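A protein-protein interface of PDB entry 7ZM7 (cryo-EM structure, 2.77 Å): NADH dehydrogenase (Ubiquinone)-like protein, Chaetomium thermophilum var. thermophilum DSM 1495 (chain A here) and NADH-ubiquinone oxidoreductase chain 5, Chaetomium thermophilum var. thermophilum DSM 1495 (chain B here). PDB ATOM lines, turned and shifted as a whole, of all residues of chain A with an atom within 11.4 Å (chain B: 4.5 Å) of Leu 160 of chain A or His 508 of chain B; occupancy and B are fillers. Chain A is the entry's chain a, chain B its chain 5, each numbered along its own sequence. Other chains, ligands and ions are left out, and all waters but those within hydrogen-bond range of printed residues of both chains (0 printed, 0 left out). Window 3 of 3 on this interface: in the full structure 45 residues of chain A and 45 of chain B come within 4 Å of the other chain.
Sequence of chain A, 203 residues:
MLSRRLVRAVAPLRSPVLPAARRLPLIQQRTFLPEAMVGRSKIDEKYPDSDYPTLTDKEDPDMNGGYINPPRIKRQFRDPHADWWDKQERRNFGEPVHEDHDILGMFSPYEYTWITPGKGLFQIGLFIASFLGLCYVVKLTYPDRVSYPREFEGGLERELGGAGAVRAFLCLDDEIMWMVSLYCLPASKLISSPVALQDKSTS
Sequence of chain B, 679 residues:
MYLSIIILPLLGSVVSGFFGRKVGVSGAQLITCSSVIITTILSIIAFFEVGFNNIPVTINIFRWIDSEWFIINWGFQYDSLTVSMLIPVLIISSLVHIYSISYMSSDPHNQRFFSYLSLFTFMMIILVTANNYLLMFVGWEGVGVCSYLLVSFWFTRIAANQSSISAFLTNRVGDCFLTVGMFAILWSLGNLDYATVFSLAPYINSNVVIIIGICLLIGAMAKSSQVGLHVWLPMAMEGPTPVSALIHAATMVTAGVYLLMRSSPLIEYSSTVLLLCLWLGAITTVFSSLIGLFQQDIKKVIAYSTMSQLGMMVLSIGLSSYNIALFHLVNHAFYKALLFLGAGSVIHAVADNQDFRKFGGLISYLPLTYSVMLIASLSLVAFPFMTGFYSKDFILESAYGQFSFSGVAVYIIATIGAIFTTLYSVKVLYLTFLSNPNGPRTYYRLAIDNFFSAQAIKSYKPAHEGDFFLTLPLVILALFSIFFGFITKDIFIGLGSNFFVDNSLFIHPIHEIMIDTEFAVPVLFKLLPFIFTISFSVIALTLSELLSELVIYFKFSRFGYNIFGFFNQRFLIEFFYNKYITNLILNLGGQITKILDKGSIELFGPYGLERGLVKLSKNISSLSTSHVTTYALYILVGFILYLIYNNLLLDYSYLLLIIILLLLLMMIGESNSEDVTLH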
ATOM      1  N   PRO A 149       9.802   4.359  29.808  1.00  0.00           N
ATOM      2  CA  PRO A 149       9.712   4.011  28.387  1.00  0.00           C
ATOM      3  C   PRO A 149       8.291   3.681  27.978  1.00  0.00           C
ATOM      4  O   PRO A 149       7.618   2.885  28.636  1.00  0.00           O
ATOM      5  CB  PRO A 149      10.626   2.789  28.258  1.00  0.00           C
ATOM      6  CG  PRO A 149      11.456   2.756  29.480  1.00  0.00           C
ATOM      7  CD  PRO A 149      10.975   3.767  30.463  1.00  0.00           C
ATOM      8  N   ARG A 150       7.830   4.283  26.887  1.00  0.00           N
ATOM      9  CA  ARG A 150       6.418   4.222  26.554  1.00  0.00           C
ATOM     10  C   ARG A 150       6.009   2.802  26.200  1.00  0.00           C
ATOM     11  O   ARG A 150       6.623   2.147  25.359  1.00  0.00           O
ATOM     12  CB  ARG A 150       6.108   5.174  25.400  1.00  0.00           C
ATOM     13  CG  ARG A 150       6.386   6.623  25.729  1.00  0.00           C
ATOM     14  CD  ARG A 150       5.953   7.549  24.612  1.00  0.00           C
ATOM     15  NE  ARG A 150       6.327   7.038  23.301  1.00  0.00           N
ATOM     16  CZ  ARG A 150       5.556   7.125  22.226  1.00  0.00           C
ATOM     17  NH1 ARG A 150       5.974   6.634  21.071  1.00  0.00           N
ATOM     18  NH2 ARG A 150       4.368   7.702  22.307  1.00  0.00           N
ATOM     19  N   GLU A 151       4.958   2.331  26.852  1.00  0.00           N
ATOM     20  CA  GLU A 151       4.468   0.983  26.644  1.00  0.00           C
ATOM     21  C   GLU A 151       3.681   0.938  25.346  1.00  0.00           C
ATOM     22  O   GLU A 151       2.789   1.761  25.124  1.00  0.00           O
ATOM     23  CB  GLU A 151       3.586   0.545  27.814  1.00  0.00           C
ATOM     24  CG  GLU A 151       3.085  -0.894  27.740  1.00  0.00           C
ATOM     25  CD  GLU A 151       4.088  -1.913  28.250  1.00  0.00           C
ATOM     26  OE1 GLU A 151       4.996  -1.537  29.021  1.00  0.00           O
ATOM     27  OE2 GLU A 151       3.965  -3.098  27.878  1.00  0.00           O
ATOM     28  N   PHE A 152       4.013  -0.022  24.497  1.00  0.00           N
ATOM     29  CA  PHE A 152       3.243  -0.300  23.301  1.00  0.00           C
ATOM     30  C   PHE A 152       2.529  -1.628  23.471  1.00  0.00           C
ATOM     31  O   PHE A 152       3.077  -2.578  24.033  1.00  0.00           O
ATOM     32  CB  PHE A 152       4.124  -0.347  22.062  1.00  0.00           C
ATOM     33  CG  PHE A 152       4.522   0.996  21.560  1.00  0.00           C
ATOM     34  CD1 PHE A 152       3.715   1.669  20.665  1.00  0.00           C
ATOM     35  CD2 PHE A 152       5.700   1.588  21.979  1.00  0.00           C
ATOM     36  CE1 PHE A 152       4.067   2.904  20.191  1.00  0.00           C
ATOM     37  CE2 PHE A 152       6.061   2.825  21.510  1.00  0.00           C
ATOM     38  CZ  PHE A 152       5.239   3.485  20.611  1.00  0.00           C
ATOM     39  N   GLU A 153       1.297  -1.685  22.983  1.00  0.00           N
ATOM     40  CA  GLU A 153       0.484  -2.886  23.121  1.00  0.00           C
ATOM     41  C   GLU A 153       0.941  -3.917  22.095  1.00  0.00           C
ATOM     42  O   GLU A 153       0.897  -3.677  20.885  1.00  0.00           O
ATOM     43  CB  GLU A 153      -0.999  -2.535  23.015  1.00  0.00           C
ATOM     44  CG  GLU A 153      -1.449  -1.910  21.713  1.00  0.00           C
ATOM     45  CD  GLU A 153      -1.789  -2.931  20.659  1.00  0.00           C
ATOM     46  OE1 GLU A 153      -2.037  -4.099  21.018  1.00  0.00           O
ATOM     47  OE2 GLU A 153      -1.787  -2.567  19.469  1.00  0.00           O
ATOM     48  N   GLY A 154       1.447  -5.043  22.590  1.00  0.00           N
ATOM     49  CA  GLY A 154       1.973  -6.101  21.757  1.00  0.00           C
ATOM     50  C   GLY A 154       3.380  -5.879  21.261  1.00  0.00           C
ATOM     51  O   GLY A 154       3.916  -6.744  20.559  1.00  0.00           O
ATOM     52  N   GLY A 155       3.996  -4.752  21.597  1.00  0.00           N
ATOM     53  CA  GLY A 155       5.334  -4.471  21.137  1.00  0.00           C
ATOM     54  C   GLY A 155       5.427  -4.041  19.695  1.00  0.00           C
ATOM     55  O   GLY A 155       6.537  -3.801  19.211  1.00  0.00           O
ATOM     56  N   LEU A 156       4.297  -3.933  18.998  1.00  0.00           N
ATOM     57  CA  LEU A 156       4.273  -3.626  17.570  1.00  0.00           C
ATOM     58  C   LEU A 156       5.141  -4.604  16.788  1.00  0.00           C
ATOM     59  O   LEU A 156       5.743  -4.258  15.771  1.00  0.00           O
ATOM     60  CB  LEU A 156       4.700  -2.185  17.303  1.00  0.00           C
ATOM     61  CG  LEU A 156       3.765  -1.110  17.843  1.00  0.00           C
ATOM     62  CD1 LEU A 156       4.359   0.263  17.616  1.00  0.00           C
ATOM     63  CD2 LEU A 156       2.402  -1.225  17.192  1.00  0.00           C
ATOM     64  N   GLU A 157       5.198  -5.846  17.266  1.00  0.00           N
ATOM     65  CA  GLU A 157       6.028  -6.846  16.613  1.00  0.00           C
ATOM     66  C   GLU A 157       5.592  -7.111  15.181  1.00  0.00           C
ATOM     67  O   GLU A 157       6.427  -7.490  14.353  1.00  0.00           O
ATOM     68  CB  GLU A 157       6.025  -8.137  17.435  1.00  0.00           C
ATOM     69  CG  GLU A 157       4.644  -8.707  17.724  1.00  0.00           C
ATOM     70  CD  GLU A 157       4.155  -9.656  16.653  1.00  0.00           C
ATOM     71  OE1 GLU A 157       4.993 -10.158  15.878  1.00  0.00           O
ATOM     72  OE2 GLU A 157       2.934  -9.909  16.594  1.00  0.00           O
ATOM     73  N   ARG A 158       4.363  -6.860  14.829  1.00  0.00           N
ATOM     74  CA  ARG A 158       3.876  -7.113  13.447  1.00  0.00           C
ATOM     75  C   ARG A 158       4.156  -5.884  12.579  1.00  0.00           C
ATOM     76  O   ARG A 158       4.119  -6.022  11.346  1.00  0.00           O
ATOM     77  CB  ARG A 158       2.385  -7.466  13.478  1.00  0.00           C
ATOM     78  CG  ARG A 158       1.958  -8.483  12.430  1.00  0.00           C
ATOM     79  CD  ARG A 158       1.300  -7.847  11.219  1.00  0.00           C
ATOM     80  NE  ARG A 158       0.113  -7.087  11.582  1.00  0.00           N
ATOM     81  CZ  ARG A 158      -1.121  -7.581  11.602  1.00  0.00           C
ATOM     82  NH1 ARG A 158      -2.137  -6.809  11.946  1.00  0.00           N
ATOM     83  NH2 ARG A 158      -1.334  -8.843  11.276  1.00  0.00           N
ATOM     84  N   GLU A 159       4.428  -4.719  13.213  1.00  0.00           N
ATOM     85  CA  GLU A 159       4.667  -3.501  12.454  1.00  0.00           C
ATOM     86  C   GLU A 159       6.139  -3.151  12.323  1.00  0.00           C
ATOM     87  O   GLU A 159       6.459  -2.038  11.907  1.00  0.00           O
ATOM     88  CB  GLU A 159       3.915  -2.335  13.093  1.00  0.00           C
ATOM     89  CG  GLU A 159       2.421  -2.401  12.881  1.00  0.00           C
ATOM     90  CD  GLU A 159       1.748  -3.345  13.850  1.00  0.00           C
ATOM     91  OE1 GLU A 159       2.441  -3.861  14.750  1.00  0.00           O
ATOM     92  OE2 GLU A 159       0.529  -3.572  13.713  1.00  0.00           O
ATOM     93  N   LEU A 160       7.043  -4.057  12.673  1.00  0.00           N
ATOM     94  CA  LEU A 160       8.467  -3.772  12.621  1.00  0.00           C
ATOM     95  C   LEU A 160       9.274  -4.896  11.997  1.00  0.00           C
ATOM     96  O   LEU A 160      10.506  -4.828  12.000  1.00  0.00           O
ATOM     97  CB  LEU A 160       9.000  -3.462  14.021  1.00  0.00           C
ATOM     98  CG  LEU A 160       8.526  -2.118  14.565  1.00  0.00           C
ATOM     99  CD1 LEU A 160       9.006  -1.890  15.980  1.00  0.00           C
ATOM    100  CD2 LEU A 160       9.005  -1.025  13.646  1.00  0.00           C
ATOM    101  N   GLY A 161       8.626  -5.920  11.464  1.00  0.00           N
ATOM    102  CA  GLY A 161       9.354  -6.963  10.777  1.00  0.00           C
ATOM    103  C   GLY A 161       9.247  -8.315  11.444  1.00  0.00           C
ATOM    104  O   GLY A 161      10.169  -9.128  11.355  1.00  0.00           O
ATOM    105  N   GLY A 162       8.134  -8.569  12.119  1.00  0.00           N
ATOM    106  CA  GLY A 162       7.926  -9.857  12.742  1.00  0.00           C
ATOM    107  C   GLY A 162       8.845 -10.076  13.923  1.00  0.00           C
ATOM    108  O   GLY A 162       9.498  -9.167  14.437  1.00  0.00           O
ATOM    109  N   ALA A 163       8.902 -11.338  14.352  1.00  0.00           N
ATOM    110  CA  ALA A 163       9.729 -11.688  15.500  1.00  0.00           C
ATOM    111  C   ALA A 163      11.215 -11.548  15.195  1.00  0.00           C
ATOM    112  O   ALA A 163      12.034 -11.503  16.119  1.00  0.00           O
ATOM    113  CB  ALA A 163       9.416 -13.112  15.953  1.00  0.00           C
ATOM    114  N   GLY A 164      11.552 -11.613  13.904  1.00  0.00           N
ATOM    115  CA  GLY A 164      12.962 -11.488  13.495  1.00  0.00           C
ATOM    116  C   GLY A 164      13.336 -10.033  13.345  1.00  0.00           C
ATOM    117  O   GLY A 164      13.993  -9.697  12.347  1.00  0.00           O
ATOM    118  N   ALA A 165      12.985  -9.211  14.333  1.00  0.00           N
ATOM    119  CA  ALA A 165      13.237  -7.757  14.231  1.00  0.00           C
ATOM    120  C   ALA A 165      13.272  -7.150  15.633  1.00  0.00           C
ATOM    121  O   ALA A 165      12.878  -7.843  16.589  1.00  0.00           O
ATOM    122  CB  ALA A 165      12.182  -7.112  13.376  1.00  0.00           C
ATOM    123  N   VAL A 166      13.778  -5.993  15.820  1.00  0.00           N
ATOM    124  CA  VAL A 166      13.774  -5.362  17.167  1.00  0.00           C
ATOM    125  C   VAL A 166      12.403  -4.715  17.392  1.00  0.00           C
ATOM    126  O   VAL A 166      11.940  -3.980  16.499  1.00  0.00           O
ATOM    127  CB  VAL A 166      14.983  -4.428  17.375  1.00  0.00           C
ATOM    128  CG1 VAL A 166      14.965  -3.198  16.482  1.00  0.00           C
ATOM    129  CG2 VAL A 166      15.175  -4.059  18.837  1.00  0.00           C
ATOM    130  N   ARG A 167      11.760  -4.978  18.461  1.00  0.00           N
ATOM    131  CA  ARG A 167      10.423  -4.533  18.821  1.00  0.00           C
ATOM    132  C   ARG A 167      10.498  -3.558  19.987  1.00  0.00           C
ATOM    133  O   ARG A 167      11.463  -3.548  20.755  1.00  0.00           O
ATOM    134  CB  ARG A 167       9.525  -5.712  19.193  1.00  0.00           C
ATOM    135  CG  ARG A 167      10.155  -6.683  20.175  1.00  0.00           C
ATOM    136  CD  ARG A 167       9.093  -7.519  20.878  1.00  0.00           C
ATOM    137  NE  ARG A 167       9.626  -8.245  22.026  1.00  0.00           N
ATOM    138  CZ  ARG A 167       9.729  -7.737  23.249  1.00  0.00           C
ATOM    139  NH1 ARG A 167       9.336  -6.495  23.488  1.00  0.00           N
ATOM    140  NH2 ARG A 167      10.224  -8.471  24.233  1.00  0.00           N
ATOM    141  N   ALA A 168       9.456  -2.745  20.124  1.00  0.00           N
ATOM    142  CA  ALA A 168       9.440  -1.702  21.138  1.00  0.00           C
ATOM    143  C   ALA A 168       9.199  -2.301  22.523  1.00  0.00           C
ATOM    144  O   ALA A 168       9.095  -3.516  22.702  1.00  0.00           O
ATOM    145  CB  ALA A 168       8.382  -0.656  20.804  1.00  0.00           C
ATOM    146  N   PHE A 169       9.114  -1.420  23.517  1.00  0.00           N
ATOM    147  CA  PHE A 169       8.974  -1.839  24.906  1.00  0.00           C
ATOM    148  C   PHE A 169       7.618  -2.493  25.145  1.00  0.00           C
ATOM    149  O   PHE A 169       6.589  -2.013  24.666  1.00  0.00           O
ATOM    150  CB  PHE A 169       9.140  -0.634  25.829  1.00  0.00           C
ATOM    151  CG  PHE A 169       9.618  -0.982  27.208  1.00  0.00           C
ATOM    152  CD1 PHE A 169      10.701  -1.821  27.387  1.00  0.00           C
ATOM    153  CD2 PHE A 169       8.989  -0.460  28.324  1.00  0.00           C
ATOM    154  CE1 PHE A 169      11.144  -2.135  28.654  1.00  0.00           C
ATOM    155  CE2 PHE A 169       9.427  -0.773  29.593  1.00  0.00           C
ATOM    156  CZ  PHE A 169      10.507  -1.612  29.758  1.00  0.00           C
ATOM    157  N   LEU A 170       7.622  -3.600  25.894  1.00  0.00           N
ATOM    158  CA  LEU A 170       6.388  -4.326  26.197  1.00  0.00           C
ATOM    159  C   LEU A 170       6.599  -5.150  27.467  1.00  0.00           C
ATOM    160  O   LEU A 170       7.172  -6.242  27.406  1.00  0.00           O
ATOM    161  CB  LEU A 170       5.981  -5.210  25.027  1.00  0.00           C
ATOM    162  CG  LEU A 170       4.822  -6.180  25.265  1.00  0.00           C
ATOM    163  CD1 LEU A 170       3.506  -5.438  25.359  1.00  0.00           C
ATOM    164  CD2 LEU A 170       4.773  -7.233  24.168  1.00  0.00           C
ATOM    165  N   PRO B 202      16.213  -4.362   8.820  1.00  0.00           N
ATOM    166  CA  PRO B 202      15.947  -4.841  10.185  1.00  0.00           C
ATOM    167  C   PRO B 202      16.494  -6.247  10.463  1.00  0.00           C
ATOM    168  O   PRO B 202      16.785  -6.530  11.604  1.00  0.00           O
ATOM    169  CB  PRO B 202      14.419  -4.932  10.280  1.00  0.00           C
ATOM    170  CG  PRO B 202      13.910  -3.950   9.262  1.00  0.00           C
ATOM    171  CD  PRO B 202      14.951  -3.941   8.169  1.00  0.00           C
ATOM    172  N   GLU B 268      19.591   3.433  11.617  1.00  0.00           N
ATOM    173  CA  GLU B 268      18.890   3.378  12.890  1.00  0.00           C
ATOM    174  C   GLU B 268      19.043   2.020  13.540  1.00  0.00           C
ATOM    175  O   GLU B 268      18.823   1.890  14.747  1.00  0.00           O
ATOM    176  CB  GLU B 268      17.411   3.649  12.693  1.00  0.00           C
ATOM    177  CG  GLU B 268      17.001   5.091  12.748  1.00  0.00           C
ATOM    178  CD  GLU B 268      16.884   5.617  14.144  1.00  0.00           C
ATOM    179  OE1 GLU B 268      17.734   6.439  14.529  1.00  0.00           O
ATOM    180  OE2 GLU B 268      15.946   5.210  14.864  1.00  0.00           O
ATOM    181  N   TYR B 269      19.395   1.003  12.760  1.00  0.00           N
ATOM    182  CA  TYR B 269      19.562  -0.350  13.253  1.00  0.00           C
ATOM    183  C   TYR B 269      20.957  -0.600  13.789  1.00  0.00           C
ATOM    184  O   TYR B 269      21.404  -1.746  13.836  1.00  0.00           O
ATOM    185  CB  TYR B 269      19.199  -1.350  12.159  1.00  0.00           C
ATOM    186  CG  TYR B 269      17.710  -1.455  11.987  1.00  0.00           C
ATOM    187  CD1 TYR B 269      16.944  -2.146  12.899  1.00  0.00           C
ATOM    188  CD2 TYR B 269      17.065  -0.844  10.922  1.00  0.00           C
ATOM    189  CE1 TYR B 269      15.587  -2.227  12.765  1.00  0.00           C
ATOM    190  CE2 TYR B 269      15.704  -0.928  10.776  1.00  0.00           C
ATOM    191  CZ  TYR B 269      14.971  -1.614  11.704  1.00  0.00           C
ATOM    192  OH  TYR B 269      13.615  -1.701  11.562  1.00  0.00           O
ATOM    193  N   PHE B 506      13.000   7.178   8.659  1.00  0.00           N
ATOM    194  CA  PHE B 506      12.501   6.166   9.574  1.00  0.00           C
ATOM    195  C   PHE B 506      13.183   6.319  10.922  1.00  0.00           C
ATOM    196  O   PHE B 506      14.408   6.207  11.024  1.00  0.00           O
ATOM    197  CB  PHE B 506      12.739   4.769   9.014  1.00  0.00           C
ATOM    198  CG  PHE B 506      12.539   3.686  10.008  1.00  0.00           C
ATOM    199  CD1 PHE B 506      11.305   3.471  10.570  1.00  0.00           C
ATOM    200  CD2 PHE B 506      13.575   2.871  10.371  1.00  0.00           C
ATOM    201  CE1 PHE B 506      11.121   2.475  11.479  1.00  0.00           C
ATOM    202  CE2 PHE B 506      13.387   1.875  11.276  1.00  0.00           C
ATOM    203  CZ  PHE B 506      12.159   1.678  11.831  1.00  0.00           C
ATOM    204  N   ILE B 507      12.396   6.577  11.953  1.00  0.00           N
ATOM    205  CA  ILE B 507      12.891   6.650  13.318  1.00  0.00           C
ATOM    206  C   ILE B 507      12.425   5.402  14.046  1.00  0.00           C
ATOM    207  O   ILE B 507      11.265   4.999  13.924  1.00  0.00           O
ATOM    208  CB  ILE B 507      12.428   7.940  14.019  1.00  0.00           C
ATOM    209  CG1 ILE B 507      10.904   8.002  14.124  1.00  0.00           C
ATOM    210  CG2 ILE B 507      12.946   9.156  13.285  1.00  0.00           C
ATOM    211  CD1 ILE B 507      10.405   9.120  14.999  1.00  0.00           C
ATOM    212  N   HIS B 508      13.333   4.738  14.761  1.00  0.00           N
ATOM    213  CA  HIS B 508      12.905   3.466  15.398  1.00  0.00           C
ATOM    214  C   HIS B 508      12.174   3.755  16.721  1.00  0.00           C
ATOM    215  O   HIS B 508      12.759   4.492  17.537  1.00  0.00           O
ATOM    216  CB  HIS B 508      14.032   2.441  15.538  1.00  0.00           C
ATOM    217  CG  HIS B 508      13.469   1.070  15.694  1.00  0.00           C
ATOM    218  ND1 HIS B 508      13.081   0.569  16.920  1.00  0.00           N
ATOM    219  CD2 HIS B 508      13.154   0.127  14.780  1.00  0.00           C
ATOM    220  CE1 HIS B 508      12.581  -0.639  16.759  1.00  0.00           C
ATOM    221  NE2 HIS B 508      12.613  -0.931  15.454  1.00  0.00           N
ATOM    222  N   PRO B 509      10.932   3.261  16.974  1.00  0.00           N
ATOM    223  CA  PRO B 509      10.218   3.594  18.214  1.00  0.00           C
ATOM    224  C   PRO B 509      10.970   3.330  19.508  1.00  0.00           C
ATOM    225  O   PRO B 509      10.494   3.759  20.560  1.00  0.00           O
ATOM    226  CB  PRO B 509       8.962   2.727  18.129  1.00  0.00           C
ATOM    227  CG  PRO B 509       8.761   2.523  16.734  1.00  0.00           C
ATOM    228  CD  PRO B 509      10.105   2.421  16.101  1.00  0.00           C
ATOM    229  N   ILE B 510      12.135   2.686  19.432  1.00  0.00           N
ATOM    230  CA  ILE B 510      12.958   2.482  20.660  1.00  0.00           C
ATOM    231  C   ILE B 510      13.835   3.716  20.912  1.00  0.00           C
ATOM    232  O   ILE B 510      14.394   3.818  22.020  1.00  0.00           O
ATOM    233  CB  ILE B 510      13.783   1.181  20.590  1.00  0.00           C
ATOM    234  CG1 ILE B 510      14.910   1.260  19.558  1.00  0.00           C
ATOM    235  CG2 ILE B 510      12.883  -0.022  20.361  1.00  0.00           C
ATOM    236  CD1 ILE B 510      15.728  -0.004  19.447  1.00  0.00           C
ATOM    237  N   HIS B 511      13.940   4.619  19.931  1.00  0.00           N
ATOM    238  CA  HIS B 511      14.734   5.876  20.126  1.00  0.00           C
ATOM    239  C   HIS B 511      14.006   7.216  20.332  1.00  0.00           C
ATOM    240  O   HIS B 511      14.666   8.119  20.873  1.00  0.00           O
ATOM    241  CB  HIS B 511      15.678   6.053  18.926  1.00  0.00           C
ATOM    242  CG  HIS B 511      16.554   4.877  18.651  1.00  0.00           C
ATOM    243  ND1 HIS B 511      16.263   3.957  17.668  1.00  0.00           N
ATOM    244  CD2 HIS B 511      17.712   4.476  19.217  1.00  0.00           C
ATOM    245  CE1 HIS B 511      17.202   3.033  17.639  1.00  0.00           C
ATOM    246  NE2 HIS B 511      18.103   3.330  18.582  1.00  0.00           N
ATOM    247  N   GLU B 512      12.668   7.367  20.194  1.00  0.00           N
ATOM    248  CA  GLU B 512      12.037   8.657  19.953  1.00  0.00           C
ATOM    249  C   GLU B 512      12.096   9.507  21.218  1.00  0.00           C
ATOM    250  O   GLU B 512      12.067   8.981  22.332  1.00  0.00           O
ATOM    251  CB  GLU B 512      10.587   8.477  19.500  1.00  0.00           C
ATOM    252  CG  GLU B 512       9.687   7.781  20.503  1.00  0.00           C
ATOM    253  CD  GLU B 512       9.094   8.733  21.517  1.00  0.00           C
ATOM    254  OE1 GLU B 512       9.067   9.951  21.242  1.00  0.00           O
ATOM    255  OE2 GLU B 512       8.650   8.263  22.586  1.00  0.00           O
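Printed residues of chain A that touch a printed residue of chain B: Arg 150, Leu 160, Val 166, Arg 167 and Ala 168.
Hydrophobic or aromatic side chains of chain A within 4 Å of the printed part of chain B: Leu 160 and Val 166.
Of the 10 printed residues of chain B, 4 touch a printed residue of chain A.
Among the printed residues, 6 pairs touch across the chains.
Among the printed residues, Asp or Glu carboxylates within 4 Å of a Lys or Arg side-chain nitrogen of the other chain: Arg 150 of chain A with Glu 512 of chain B (2.7 Å).
Leu 160 of chain A touches His 508 of chain B (CD1 to NE2, 3.8 Å).
Val 166 of chain A touches Tyr 269 of chain B (CG1 to CE1, 3.9 Å).
Arg 167 of chain A touches Ile 510 of chain B.
Ile 510 of chain B touches Ala 168 of chain A.
Pro 202 of chain B touches none of the printed residues of chain A.
No residue of chain A comes within 4 Å of Phe 506 of chain B.
No residue of chain A comes within 4 Å of Pro 509 of chain B.
Of chain A, only Arg 167 (3.8 Å) and Ala 168 (3.9 Å) come within 4 Å of Ile 510 of chain B.
His 511 of chain B touches none of the printed residues of chain A.
Printed residues of chain B within 4 Å of Val 166 of chain A: Tyr 269 (3.9 Å) and His 508 (3.3 Å).
Printed residues of chain B within 4 Å of Ala 168 of chain A: Ile 510.
Of the printed residues of chain B, Arg 150 of chain A touches Glu 512.
Leu 156 of chain A touches none of the printed residues of chain B.
The nearest residue of chain B that does not touch Leu 160 of chain A is Pro 202 of chain B (4.3 Å).
The nearest residue of chain A that does not touch His 508 of chain B is Arg 167 of chain A (4.7 Å).
The nearest printed residue of chain B that does not touch Val 166 of chain A is Ile 510 of chain B (4.1 Å).
The backbone carbonyl oxygen of Gly 155 of chain A sits at hydrogen-bond distance from the backbone NH of Ala 168 of chain A, 3.2 Å away.
N of His 508 of chain B lies within hydrogen-bond range of OE2 of Glu 268 of chain B.
The backbone NH of Ile 510 of chain B sits close to a ring nitrogen (ND1) of His 508 of chain B (3.4 Å).
The guanidinium group (NE) of Arg 150 of chain A lies within salt-bridge range of the side-chain carboxylate (OE2) of Glu 512 of chain B (2.7 Å).
The backbone carbonyl oxygen (O) of Val 166 of chain A is in hydrogen-bond range of a ring nitrogen (NE2) of His 508 of chain B, at 3.3 Å.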
